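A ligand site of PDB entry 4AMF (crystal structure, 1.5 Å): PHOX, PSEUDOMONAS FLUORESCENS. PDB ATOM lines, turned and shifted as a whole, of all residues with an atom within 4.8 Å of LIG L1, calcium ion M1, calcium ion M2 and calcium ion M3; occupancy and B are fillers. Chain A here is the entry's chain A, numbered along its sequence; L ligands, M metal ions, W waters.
Merely in contact with calcium ion M1: Cys 175 and Trp 384.
The backbone carbonyl oxygen (O) of Glu 528 is in hydrogen-bond range of the backbone NH (N) of Gln 546, at 3.0 Å.
The side-chain carboxylate of Glu 528 sits close to a ring nitrogen (NE2) of His 547 (2.6 Å).
The backbone carbonyl oxygen (O) of Asp 475 is in hydrogen-bond range of the backbone NH (N) of Trp 384 (3.3 Å).
OE2 of Glu 383 sits close to NH2 of Arg 381 (3.95 Å).
The side-chain carboxylate (OD1) of Asp 288 is in salt-bridge range of the guanidinium group (NE) of Arg 381, at 2.9 Å.
O of Arg 381 sits at hydrogen-bond distance from N of Thr 399 (3.1 Å).
The side-chain carboxylate (OE1) of Glu 190 lies close to the side-chain amide nitrogen (ND2) of Asn 191 (3.4 Å).
The side-chain carboxylate (OE1) of Glu 86 lies within hydrogen-bond range of the side-chain amide nitrogen (NE2) of Gln 546 (3.3 Å).
Two residues have an atom within 4 Å of calcium ion M3: Asp 490 and Glu 528.
An oxygen (O2) of LIG L1 sits close to the side-chain carboxylate (OE2) of Glu 86, at 3.0 Å.
OE1 of Glu 190 sits close to O2 of LIG L1 (2.9 Å).
The side-chain carboxylate (OD2) of Asp 288 lies close to an oxygen (O3) of LIG L1 (2.7 Å).
Arg 219 touches LIG L1 (NE to C9, 3.4 Å).
Within 4 Å of LIG L1: Glu 86, Glu 190, Asn 191, Arg 219, Asp 288, Arg 290, Arg 381, Glu 383, Asp 475, Asp 490 and Glu 528.
Along chain A the residues within 4 Å of LIG L1 span positions 86 to 528.
Arg 381 touches calcium ion M2.
Within 4 Å of calcium ion M2: Arg 381, Glu 383, Asp 475 and Asp 490.
The nearest printed residue that does not touch calcium ion M2 is Asp 288 (4.6 Å).
An oxygen (O1) of LIG L1 binds calcium ion M3 (2.3 Å).
Calcium ion M3 is bound by OE1 of Glu 528.
Calcium ion M3 is bound by OD2 of Asp 490, at 2.3 Å.
Water W7 is bound to calcium ion M3, 2.4 Å away.
O5 of LIG L1 is bound to calcium ion M3 (2.5 Å).
Water W9 is bound to calcium ion M3 (2.5 Å).
Calcium ion M3 is bound by OE2 of Glu 528 (2.8 Å).
Calcium ion M3 has seven donor atoms within binding distance.
NE of Arg 381 sits at hydrogen-bond distance from O11 of LIG L1, 3.3 Å away.
NH2 of Arg 290 sits at hydrogen-bond distance from O10 of LIG L1 (3.4 Å).
An oxygen (O12) of LIG L1 is in hydrogen-bond range of the side-chain amide oxygen of Asn 191 (3.5 Å).
The side-chain carboxylate of Glu 269 binds an iron atom (FE2) of LG2 L2 (2.1 Å).
OE2 of Glu 383 is bound to FE2 of LG2 L2 (2.1 Å).
An iron atom (FE2) of LG2 L2 is bound by the side-chain carboxylate of Asp 288.
An iron atom (FE2) of LG2 L2 is bound by the side-chain carboxylate of Glu 190, at 2.0 Å.
The side-chain carboxylate (OE2) of Glu 86 is bound to an iron atom (FE1) of LG2 L2 (2.0 Å).
The side-chain sulfur of Cys 175 binds an iron atom (FE1) of LG2 L2, 2.6 Å away.
Water W13 lies within hydrogen-bond range of OD2 of Asp 65 (2.6 Å) and OE1 of Glu 86 (3.1 Å).
Water W6 bridges OG1 of Thr 399 (2.8 Å) and O of Asp 490 (2.9 Å).
Water W16 lies within hydrogen-bond range of an oxygen (O11) of LIG L1, the backbone carbonyl oxygen (O) of Asp 288, the side-chain amide nitrogen (ND2) of Asn 191 and the guanidinium group (NH2) of Arg 381.
Water W10 bridges O11 of LIG L1 (2.8 Å) and N of Arg 290 (2.9 Å).
Water W1 lies within hydrogen-bond range of the guanidinium group (NH1) of Arg 219 and an oxygen (O12) of LIG L1.
Water W8 lies within hydrogen-bond range of OD1 of Asn 191 (2.7 Å), O of Asp 288 (2.8 Å) and O12 of LIG L1 (2.9 Å).
Calcium ion M1 is bound by an oxygen (O1) of LG2 L2 (2.2 Å), the side-chain carboxylate (OE2) of Glu 269 (2.3 Å), the side-chain carboxylate (OD1) of Asp 475 (2.4 Å), the side-chain carboxylate (OD2) of Asp 475 (2.4 Å), water W12 (2.5 Å), water W15 (2.6 Å) and water W13 (2.7 Å).
Calcium ion M1 has seven donor atoms within binding distance.
Slightly farther from calcium ion M1 lies the side-chain carboxylate (OE2) of Glu 383 (2.9 Å).
FE2 of LG2 L2 is bound by O3 of LIG L1.
Calcium ion M2 is bound by water W6 (2.3 Å).
The side-chain carboxylate (OD2) of Asp 475 binds calcium ion M2.
OD2 of Asp 490 is bound to calcium ion M2.
Calcium ion M2 is bound by an oxygen (O1) of LIG L1 (2.4 Å).
O4 of LIG L1 is bound to calcium ion M2 (2.5 Å).
The side-chain carboxylate (OE2) of Glu 383 is bound to calcium ion M2 (2.6 Å).
The side-chain carboxylate (OE1) of Glu 383 is bound to calcium ion M2 (2.7 Å).
Calcium ion M2 has seven donor atoms within binding distance.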
ATOM      1  N   ASP A  65      25.624  16.960   7.343  1.00  0.00           N
ATOM      2  CA  ASP A  65      26.303  16.598   6.100  1.00  0.00           C
ATOM      3  C   ASP A  65      26.860  17.851   5.408  1.00  0.00           C
ATOM      4  O   ASP A  65      27.582  18.586   6.054  1.00  0.00           O
ATOM      5  CB  ASP A  65      25.319  15.735   5.288  1.00  0.00           C
ATOM      6  CG  ASP A  65      25.872  14.836   4.229  1.00  0.00           C
ATOM      7  OD1 ASP A  65      26.993  15.066   3.783  1.00  0.00           O
ATOM      8  OD2 ASP A  65      25.199  13.828   3.908  1.00  0.00           O
ATOM      9  N   GLU A  86      20.939  15.057   6.900  1.00  0.00           N
ATOM     10  CA  GLU A  86      20.565  14.101   5.850  1.00  0.00           C
ATOM     11  C   GLU A  86      19.558  13.051   6.216  1.00  0.00           C
ATOM     12  O   GLU A  86      18.649  12.773   5.421  1.00  0.00           O
ATOM     13  CB  GLU A  86      21.855  13.451   5.275  1.00  0.00           C
ATOM     14  CG  GLU A  86      21.562  12.656   3.999  1.00  0.00           C
ATOM     15  CD  GLU A  86      22.698  11.853   3.422  1.00  0.00           C
ATOM     16  OE1 GLU A  86      23.459  11.252   4.210  1.00  0.00           O
ATOM     17  OE2 GLU A  86      22.899  11.932   2.201  1.00  0.00           O
ATOM     18  N   CYS A 175      21.605  16.006   1.375  1.00  0.00           N
ATOM     19  CA  CYS A 175      22.920  15.424   1.335  1.00  0.00           C
ATOM     20  C   CYS A 175      23.985  16.486   1.353  1.00  0.00           C
ATOM     21  O   CYS A 175      24.419  16.961   2.429  1.00  0.00           O
ATOM     22  CB  CYS A 175      22.994  14.517   0.121  1.00  0.00           C
ATOM     23  SG  CYS A 175      24.589  13.783  -0.157  1.00  0.00           S
ATOM     24  N   GLU A 190      18.906  13.872  -2.072  1.00  0.00           N
ATOM     25  CA  GLU A 190      19.568  12.705  -2.640  1.00  0.00           C
ATOM     26  C   GLU A 190      18.699  11.462  -2.544  1.00  0.00           C
ATOM     27  O   GLU A 190      17.877  11.220  -3.449  1.00  0.00           O
ATOM     28  CB  GLU A 190      20.936  12.514  -2.007  1.00  0.00           C
ATOM     29  CG  GLU A 190      21.764  11.405  -2.633  1.00  0.00           C
ATOM     30  CD  GLU A 190      22.910  10.962  -1.754  1.00  0.00           C
ATOM     31  OE1 GLU A 190      22.807  11.126  -0.512  1.00  0.00           O
ATOM     32  OE2 GLU A 190      23.942  10.504  -2.296  1.00  0.00           O
ATOM     33  N   ASN A 191      18.805  10.652  -1.477  1.00  0.00           N
ATOM     34  CA  ASN A 191      18.061   9.382  -1.409  1.00  0.00           C
ATOM     35  C   ASN A 191      16.615   9.552  -0.927  1.00  0.00           C
ATOM     36  O   ASN A 191      16.132   8.812  -0.074  1.00  0.00           O
ATOM     37  CB  ASN A 191      18.845   8.365  -0.588  1.00  0.00           C
ATOM     38  CG  ASN A 191      20.071   7.900  -1.365  1.00  0.00           C
ATOM     39  OD1 ASN A 191      19.944   7.463  -2.509  1.00  0.00           O
ATOM     40  ND2 ASN A 191      21.269   8.083  -0.823  1.00  0.00           N
ATOM     41  N   ARG A 219      12.737   1.939   1.876  1.00  0.00           N
ATOM     42  CA  ARG A 219      14.063   1.418   2.140  1.00  0.00           C
ATOM     43  C   ARG A 219      14.337   1.543   3.630  1.00  0.00           C
ATOM     44  O   ARG A 219      15.167   2.363   4.057  1.00  0.00           O
ATOM     45  CB  ARG A 219      15.133   2.108   1.275  1.00  0.00           C
ATOM     46  CG  ARG A 219      16.469   1.353   1.270  1.00  0.00           C
ATOM     47  CD  ARG A 219      17.396   1.872   0.213  1.00  0.00           C
ATOM     48  NE  ARG A 219      16.925   1.568  -1.137  1.00  0.00           N
ATOM     49  CZ  ARG A 219      17.385   2.130  -2.254  1.00  0.00           C
ATOM     50  NH1 ARG A 219      18.339   3.050  -2.206  1.00  0.00           N
ATOM     51  NH2 ARG A 219      16.876   1.797  -3.431  1.00  0.00           N
ATOM     52  N   GLU A 269      23.615  14.956  -5.131  1.00  0.00           N
ATOM     53  CA  GLU A 269      24.601  14.971  -4.060  1.00  0.00           C
ATOM     54  C   GLU A 269      24.956  16.413  -3.674  1.00  0.00           C
ATOM     55  O   GLU A 269      24.588  16.846  -2.607  1.00  0.00           O
ATOM     56  CB  GLU A 269      25.867  14.204  -4.438  1.00  0.00           C
ATOM     57  CG  GLU A 269      26.884  14.162  -3.304  1.00  0.00           C
ATOM     58  CD  GLU A 269      26.922  12.904  -2.499  1.00  0.00           C
ATOM     59  OE1 GLU A 269      26.295  11.909  -2.911  1.00  0.00           O
ATOM     60  OE2 GLU A 269      27.531  12.946  -1.399  1.00  0.00           O
ATOM     61  N   ASP A 288      23.829  10.510  -7.312  1.00  0.00           N
ATOM     62  CA  ASP A 288      24.534   9.451  -6.621  1.00  0.00           C
ATOM     63  C   ASP A 288      23.781   8.133  -6.556  1.00  0.00           C
ATOM     64  O   ASP A 288      23.135   7.775  -5.573  1.00  0.00           O
ATOM     65  CB  ASP A 288      25.018   9.868  -5.256  1.00  0.00           C
ATOM     66  CG  ASP A 288      25.845   8.766  -4.611  1.00  0.00           C
ATOM     67  OD1 ASP A 288      26.255   7.840  -5.334  1.00  0.00           O
ATOM     68  OD2 ASP A 288      26.040   8.802  -3.412  1.00  0.00           O
ATOM     69  N   GLU A 289      23.973   7.388  -7.597  1.00  0.00           N
ATOM     70  CA  GLU A 289      23.464   6.011  -7.701  1.00  0.00           C
ATOM     71  C   GLU A 289      24.360   5.237  -8.678  1.00  0.00           C
ATOM     72  O   GLU A 289      24.784   5.775  -9.698  1.00  0.00           O
ATOM     73  CB  GLU A 289      21.989   5.953  -8.088  1.00  0.00           C
ATOM     74  CG  GLU A 289      21.421   4.537  -8.059  1.00  0.00           C
ATOM     75  CD  GLU A 289      19.919   4.454  -8.178  1.00  0.00           C
ATOM     76  OE1 GLU A 289      19.239   5.436  -7.787  1.00  0.00           O
ATOM     77  OE2 GLU A 289      19.408   3.406  -8.642  1.00  0.00           O
ATOM     78  N   ARG A 290      24.692   4.001  -8.336  1.00  0.00           N
ATOM     79  CA  ARG A 290      25.499   3.190  -9.249  1.00  0.00           C
ATOM     80  C   ARG A 290      24.957   3.250 -10.698  1.00  0.00           C
ATOM     81  O   ARG A 290      23.781   2.984 -10.943  1.00  0.00           O
ATOM     82  CB  ARG A 290      25.503   1.713  -8.821  1.00  0.00           C
ATOM     83  CG  ARG A 290      26.325   1.388  -7.591  1.00  0.00           C
ATOM     84  CD  ARG A 290      26.290  -0.105  -7.321  1.00  0.00           C
ATOM     85  NE  ARG A 290      25.068  -0.506  -6.645  1.00  0.00           N
ATOM     86  CZ  ARG A 290      24.893  -0.508  -5.326  1.00  0.00           C
ATOM     87  NH1 ARG A 290      25.877  -0.126  -4.504  1.00  0.00           N
ATOM     88  NH2 ARG A 290      23.746  -0.881  -4.798  1.00  0.00           N
ATOM     89  N   ARG A 381      28.939   6.114  -9.300  1.00  0.00           N
ATOM     90  CA  ARG A 381      28.430   6.887  -8.168  1.00  0.00           C
ATOM     91  C   ARG A 381      29.054   8.259  -7.956  1.00  0.00           C
ATOM     92  O   ARG A 381      29.864   8.462  -7.049  1.00  0.00           O
ATOM     93  CB  ARG A 381      28.546   6.078  -6.885  1.00  0.00           C
ATOM     94  CG  ARG A 381      27.600   4.891  -6.834  1.00  0.00           C
ATOM     95  CD  ARG A 381      27.641   4.296  -5.468  1.00  0.00           C
ATOM     96  NE  ARG A 381      27.141   5.265  -4.493  1.00  0.00           N
ATOM     97  CZ  ARG A 381      27.343   5.213  -3.181  1.00  0.00           C
ATOM     98  NH1 ARG A 381      28.006   4.193  -2.642  1.00  0.00           N
ATOM     99  NH2 ARG A 381      26.872   6.168  -2.391  1.00  0.00           N
ATOM    100  N   GLU A 383      29.609  11.578  -6.403  1.00  0.00           N
ATOM    101  CA  GLU A 383      29.241  12.242  -5.170  1.00  0.00           C
ATOM    102  C   GLU A 383      29.637  13.723  -5.303  1.00  0.00           C
ATOM    103  O   GLU A 383      29.113  14.361  -6.222  1.00  0.00           O
ATOM    104  CB  GLU A 383      29.704  11.490  -3.919  1.00  0.00           C
ATOM    105  CG  GLU A 383      28.914  10.197  -3.742  1.00  0.00           C
ATOM    106  CD  GLU A 383      28.901   9.622  -2.335  1.00  0.00           C
ATOM    107  OE1 GLU A 383      29.905   8.967  -1.986  1.00  0.00           O
ATOM    108  OE2 GLU A 383      27.961   9.870  -1.546  1.00  0.00           O
ATOM    109  N   TRP A 384      30.469  14.297  -4.450  1.00  0.00           N
ATOM    110  CA  TRP A 384      30.693  15.733  -4.507  1.00  0.00           C
ATOM    111  C   TRP A 384      31.505  16.147  -5.708  1.00  0.00           C
ATOM    112  O   TRP A 384      32.476  15.480  -6.079  1.00  0.00           O
ATOM    113  CB  TRP A 384      31.371  16.264  -3.248  1.00  0.00           C
ATOM    114  CG  TRP A 384      30.549  16.201  -2.012  1.00  0.00           C
ATOM    115  CD1 TRP A 384      29.841  15.136  -1.562  1.00  0.00           C
ATOM    116  CD2 TRP A 384      30.641  17.110  -0.908  1.00  0.00           C
ATOM    117  NE1 TRP A 384      29.375  15.370  -0.301  1.00  0.00           N
ATOM    118  CE2 TRP A 384      29.934  16.520   0.175  1.00  0.00           C
ATOM    119  CE3 TRP A 384      31.254  18.359  -0.715  1.00  0.00           C
ATOM    120  CZ2 TRP A 384      29.826  17.140   1.407  1.00  0.00           C
ATOM    121  CZ3 TRP A 384      31.241  18.900   0.551  1.00  0.00           C
ATOM    122  CH2 TRP A 384      30.477  18.333   1.573  1.00  0.00           C
ATOM    123  N   THR A 399      32.542   7.392  -5.934  1.00  0.00           N
ATOM    124  CA  THR A 399      32.815   6.755  -4.639  1.00  0.00           C
ATOM    125  C   THR A 399      33.093   5.286  -4.660  1.00  0.00           C
ATOM    126  O   THR A 399      34.005   4.836  -3.962  1.00  0.00           O
ATOM    127  CB  THR A 399      31.789   7.157  -3.583  1.00  0.00           C
ATOM    128  OG1 THR A 399      32.378   6.965  -2.279  1.00  0.00           O
ATOM    129  CG2 THR A 399      30.504   6.448  -3.729  1.00  0.00           C
ATOM    130  N   ASP A 475      34.081  10.781  -0.918  1.00  0.00           N
ATOM    131  CA  ASP A 475      32.706  11.242  -1.025  1.00  0.00           C
ATOM    132  C   ASP A 475      32.759  12.755  -1.090  1.00  0.00           C
ATOM    133  O   ASP A 475      32.695  13.322  -2.202  1.00  0.00           O
ATOM    134  CB  ASP A 475      31.920  10.618   0.124  1.00  0.00           C
ATOM    135  CG  ASP A 475      30.470  11.039   0.239  1.00  0.00           C
ATOM    136  OD1 ASP A 475      30.132  12.126  -0.227  1.00  0.00           O
ATOM    137  OD2 ASP A 475      29.670  10.252   0.793  1.00  0.00           O
ATOM    138  N   ASP A 490      33.760   8.331   3.059  1.00  0.00           N
ATOM    139  CA  ASP A 490      32.590   7.622   3.499  1.00  0.00           C
ATOM    140  C   ASP A 490      32.690   6.209   2.995  1.00  0.00           C
ATOM    141  O   ASP A 490      31.909   5.775   2.151  1.00  0.00           O
ATOM    142  CB  ASP A 490      31.302   8.295   2.978  1.00  0.00           C
ATOM    143  CG  ASP A 490      30.049   7.502   3.300  1.00  0.00           C
ATOM    144  OD1 ASP A 490      30.050   6.746   4.308  1.00  0.00           O
ATOM    145  OD2 ASP A 490      29.053   7.631   2.541  1.00  0.00           O
ATOM    146  N   GLU A 528      31.106   8.663   9.195  1.00  0.00           N
ATOM    147  CA  GLU A 528      31.684   9.121   7.965  1.00  0.00           C
ATOM    148  C   GLU A 528      32.091  10.592   8.212  1.00  0.00           C
ATOM    149  O   GLU A 528      31.521  11.243   9.106  1.00  0.00           O
ATOM    150  CB  GLU A 528      30.830   8.941   6.727  1.00  0.00           C
ATOM    151  CG  GLU A 528      29.597   9.814   6.655  1.00  0.00           C
ATOM    152  CD  GLU A 528      28.695   9.377   5.528  1.00  0.00           C
ATOM    153  OE1 GLU A 528      28.023   8.339   5.713  1.00  0.00           O
ATOM    154  OE2 GLU A 528      28.701  10.019   4.451  1.00  0.00           O
ATOM    155  N   THR A 530      32.076  14.162   6.649  1.00  0.00           N
ATOM    156  CA  THR A 530      31.310  14.841   5.584  1.00  0.00           C
ATOM    157  C   THR A 530      30.998  16.275   5.981  1.00  0.00           C
ATOM    158  O   THR A 530      30.875  16.575   7.168  1.00  0.00           O
ATOM    159  CB  THR A 530      30.067  14.001   5.215  1.00  0.00           C
ATOM    160  OG1 THR A 530      29.425  14.596   4.095  1.00  0.00           O
ATOM    161  CG2 THR A 530      29.098  13.835   6.352  1.00  0.00           C
ATOM    162  N   GLN A 546      29.418  12.458  10.850  1.00  0.00           N
ATOM    163  CA  GLN A 546      28.066  11.966  10.643  1.00  0.00           C
ATOM    164  C   GLN A 546      27.900  10.544  11.130  1.00  0.00           C
ATOM    165  O   GLN A 546      28.761   9.695  10.892  1.00  0.00           O
ATOM    166  CB  GLN A 546      27.704  12.087   9.161  1.00  0.00           C
ATOM    167  CG  GLN A 546      26.228  11.994   8.869  1.00  0.00           C
ATOM    168  CD  GLN A 546      25.919  11.710   7.418  1.00  0.00           C
ATOM    169  OE1 GLN A 546      26.496  10.808   6.823  1.00  0.00           O
ATOM    170  NE2 GLN A 546      25.013  12.479   6.808  1.00  0.00           N
ATOM    171  N   HIS A 547      26.793  10.288  11.801  1.00  0.00           N
ATOM    172  CA  HIS A 547      26.411   9.012  12.371  1.00  0.00           C
ATOM    173  C   HIS A 547      27.529   8.259  13.108  1.00  0.00           C
ATOM    174  O   HIS A 547      27.721   7.071  12.887  1.00  0.00           O
ATOM    175  CB  HIS A 547      25.731   8.121  11.319  1.00  0.00           C
ATOM    176  CG  HIS A 547      26.578   7.751  10.130  1.00  0.00           C
ATOM    177  ND1 HIS A 547      27.621   6.859  10.234  1.00  0.00           N
ATOM    178  CD2 HIS A 547      26.505   8.176   8.853  1.00  0.00           C
ATOM    179  CE1 HIS A 547      28.144   6.743   9.028  1.00  0.00           C
ATOM    180  NE2 HIS A 547      27.507   7.521   8.151  1.00  0.00           N
HETATM  181  P1  LIG L   1      25.392   8.380   0.738  1.00  0.00           P
HETATM  182  O1  LIG L   1      26.733   8.748   1.513  1.00  0.00           O
HETATM  183  O2  LIG L   1      24.191   9.360   1.289  1.00  0.00           O
HETATM  184  O3  LIG L   1      25.600   8.437  -0.810  1.00  0.00           O
HETATM  185  P2  LIG L   1      26.383   5.687   1.232  1.00  0.00           P
HETATM  186  O4  LIG L   1      27.421   6.025   0.236  1.00  0.00           O
HETATM  187  O5  LIG L   1      26.723   5.639   2.739  1.00  0.00           O
HETATM  188  C1  LIG L   1      24.961   6.682   1.027  1.00  0.00           C
HETATM  189  P3  LIG L   1      25.565   2.900   1.429  1.00  0.00           P
HETATM  190  O6  LIG L   1      24.481   3.115   2.405  1.00  0.00           O
HETATM  191  O7  LIG L   1      26.761   2.068   1.747  1.00  0.00           O
HETATM  192  O8  LIG L   1      26.014   4.231   0.769  1.00  0.00           O
HETATM  193  O9  LIG L   1      24.936   2.095   0.121  1.00  0.00           O
HETATM  194  C2  LIG L   1      25.645   2.024  -1.126  1.00  0.00           C
HETATM  195  C3  LIG L   1      24.795   2.537  -2.261  1.00  0.00           C
HETATM  196  O10 LIG L   1      23.723   1.603  -2.496  1.00  0.00           O
HETATM  197  C4  LIG L   1      24.130   3.904  -2.120  1.00  0.00           C
HETATM  198  O11 LIG L   1      24.134   4.580  -3.385  1.00  0.00           O
HETATM  199  C5  LIG L   1      22.731   3.553  -1.613  1.00  0.00           C
HETATM  200  O12 LIG L   1      21.799   4.572  -1.947  1.00  0.00           O
HETATM  201  C6  LIG L   1      22.459   2.225  -2.340  1.00  0.00           C
HETATM  202  N1  LIG L   1      21.586   1.306  -1.635  1.00  0.00           N
HETATM  203  C7  LIG L   1      21.506   1.086  -0.286  1.00  0.00           C
HETATM  204  N2  LIG L   1      20.617   0.177   0.062  1.00  0.00           N
HETATM  205  C8  LIG L   1      20.079  -0.232  -1.145  1.00  0.00           C
HETATM  206  C9  LIG L   1      19.039  -1.137  -1.464  1.00  0.00           C
HETATM  207  N3  LIG L   1      18.289  -1.756  -0.559  1.00  0.00           N
HETATM  208  N4  LIG L   1      18.750  -1.309  -2.776  1.00  0.00           N
HETATM  209  C10 LIG L   1      19.421  -0.606  -3.690  1.00  0.00           C
HETATM  210  N5  LIG L   1      20.405   0.285  -3.496  1.00  0.00           N
HETATM  211  C11 LIG L   1      20.680   0.440  -2.205  1.00  0.00           C
HETATM  212 FE1  LG2 L   2      24.352  11.437   0.883  1.00  0.00          FE
HETATM  213 FE2  LG2 L   2      25.905  10.185  -1.841  1.00  0.00          FE
HETATM  214  O1  LG2 L   2      25.968  11.100  -0.113  1.00  0.00           O
HETATM  215 CA    CA M   1      27.928  11.883   0.600  1.00  0.00          CA
HETATM  216 CA    CA M   2      28.686   8.171   0.237  1.00  0.00          CA
HETATM  217 CA    CA M   3      27.014   7.931   3.665  1.00  0.00          CA
HETATM  218  O   HOH W   1      19.634   4.351  -0.020  1.00  0.00           O
HETATM  219  O   HOH W   2      23.743   4.667   4.253  1.00  0.00           O
HETATM  220  O   HOH W   3      21.450   1.722  -5.715  1.00  0.00           O
HETATM  221  O   HOH W   4      27.163   1.785   4.538  1.00  0.00           O
HETATM  222  O   HOH W   5      29.619   3.877  -0.246  1.00  0.00           O
HETATM  223  O   HOH W   6      30.517   6.831  -0.191  1.00  0.00           O
HETATM  224  O   HOH W   7      25.641   9.827   4.319  1.00  0.00           O
HETATM  225  O   HOH W   8      21.240   6.042  -4.425  1.00  0.00           O
HETATM  226  O   HOH W   9      25.311   6.747   5.070  1.00  0.00           O
HETATM  227  O   HOH W  10      23.886   3.084  -5.747  1.00  0.00           O
HETATM  228  O   HOH W  11      21.703   8.676   1.931  1.00  0.00           O
HETATM  229  O   HOH W  12      29.008  12.171   2.794  1.00  0.00           O
HETATM  230  O   HOH W  13      26.016  11.841   2.472  1.00  0.00           O
HETATM  231  O   HOH W  14      28.735   4.258   3.773  1.00  0.00           O
HETATM  232  O   HOH W  15      27.269  14.289   1.341  1.00  0.00           O
HETATM  233  O   HOH W  16      23.739   7.227  -2.610  1.00  0.00           O
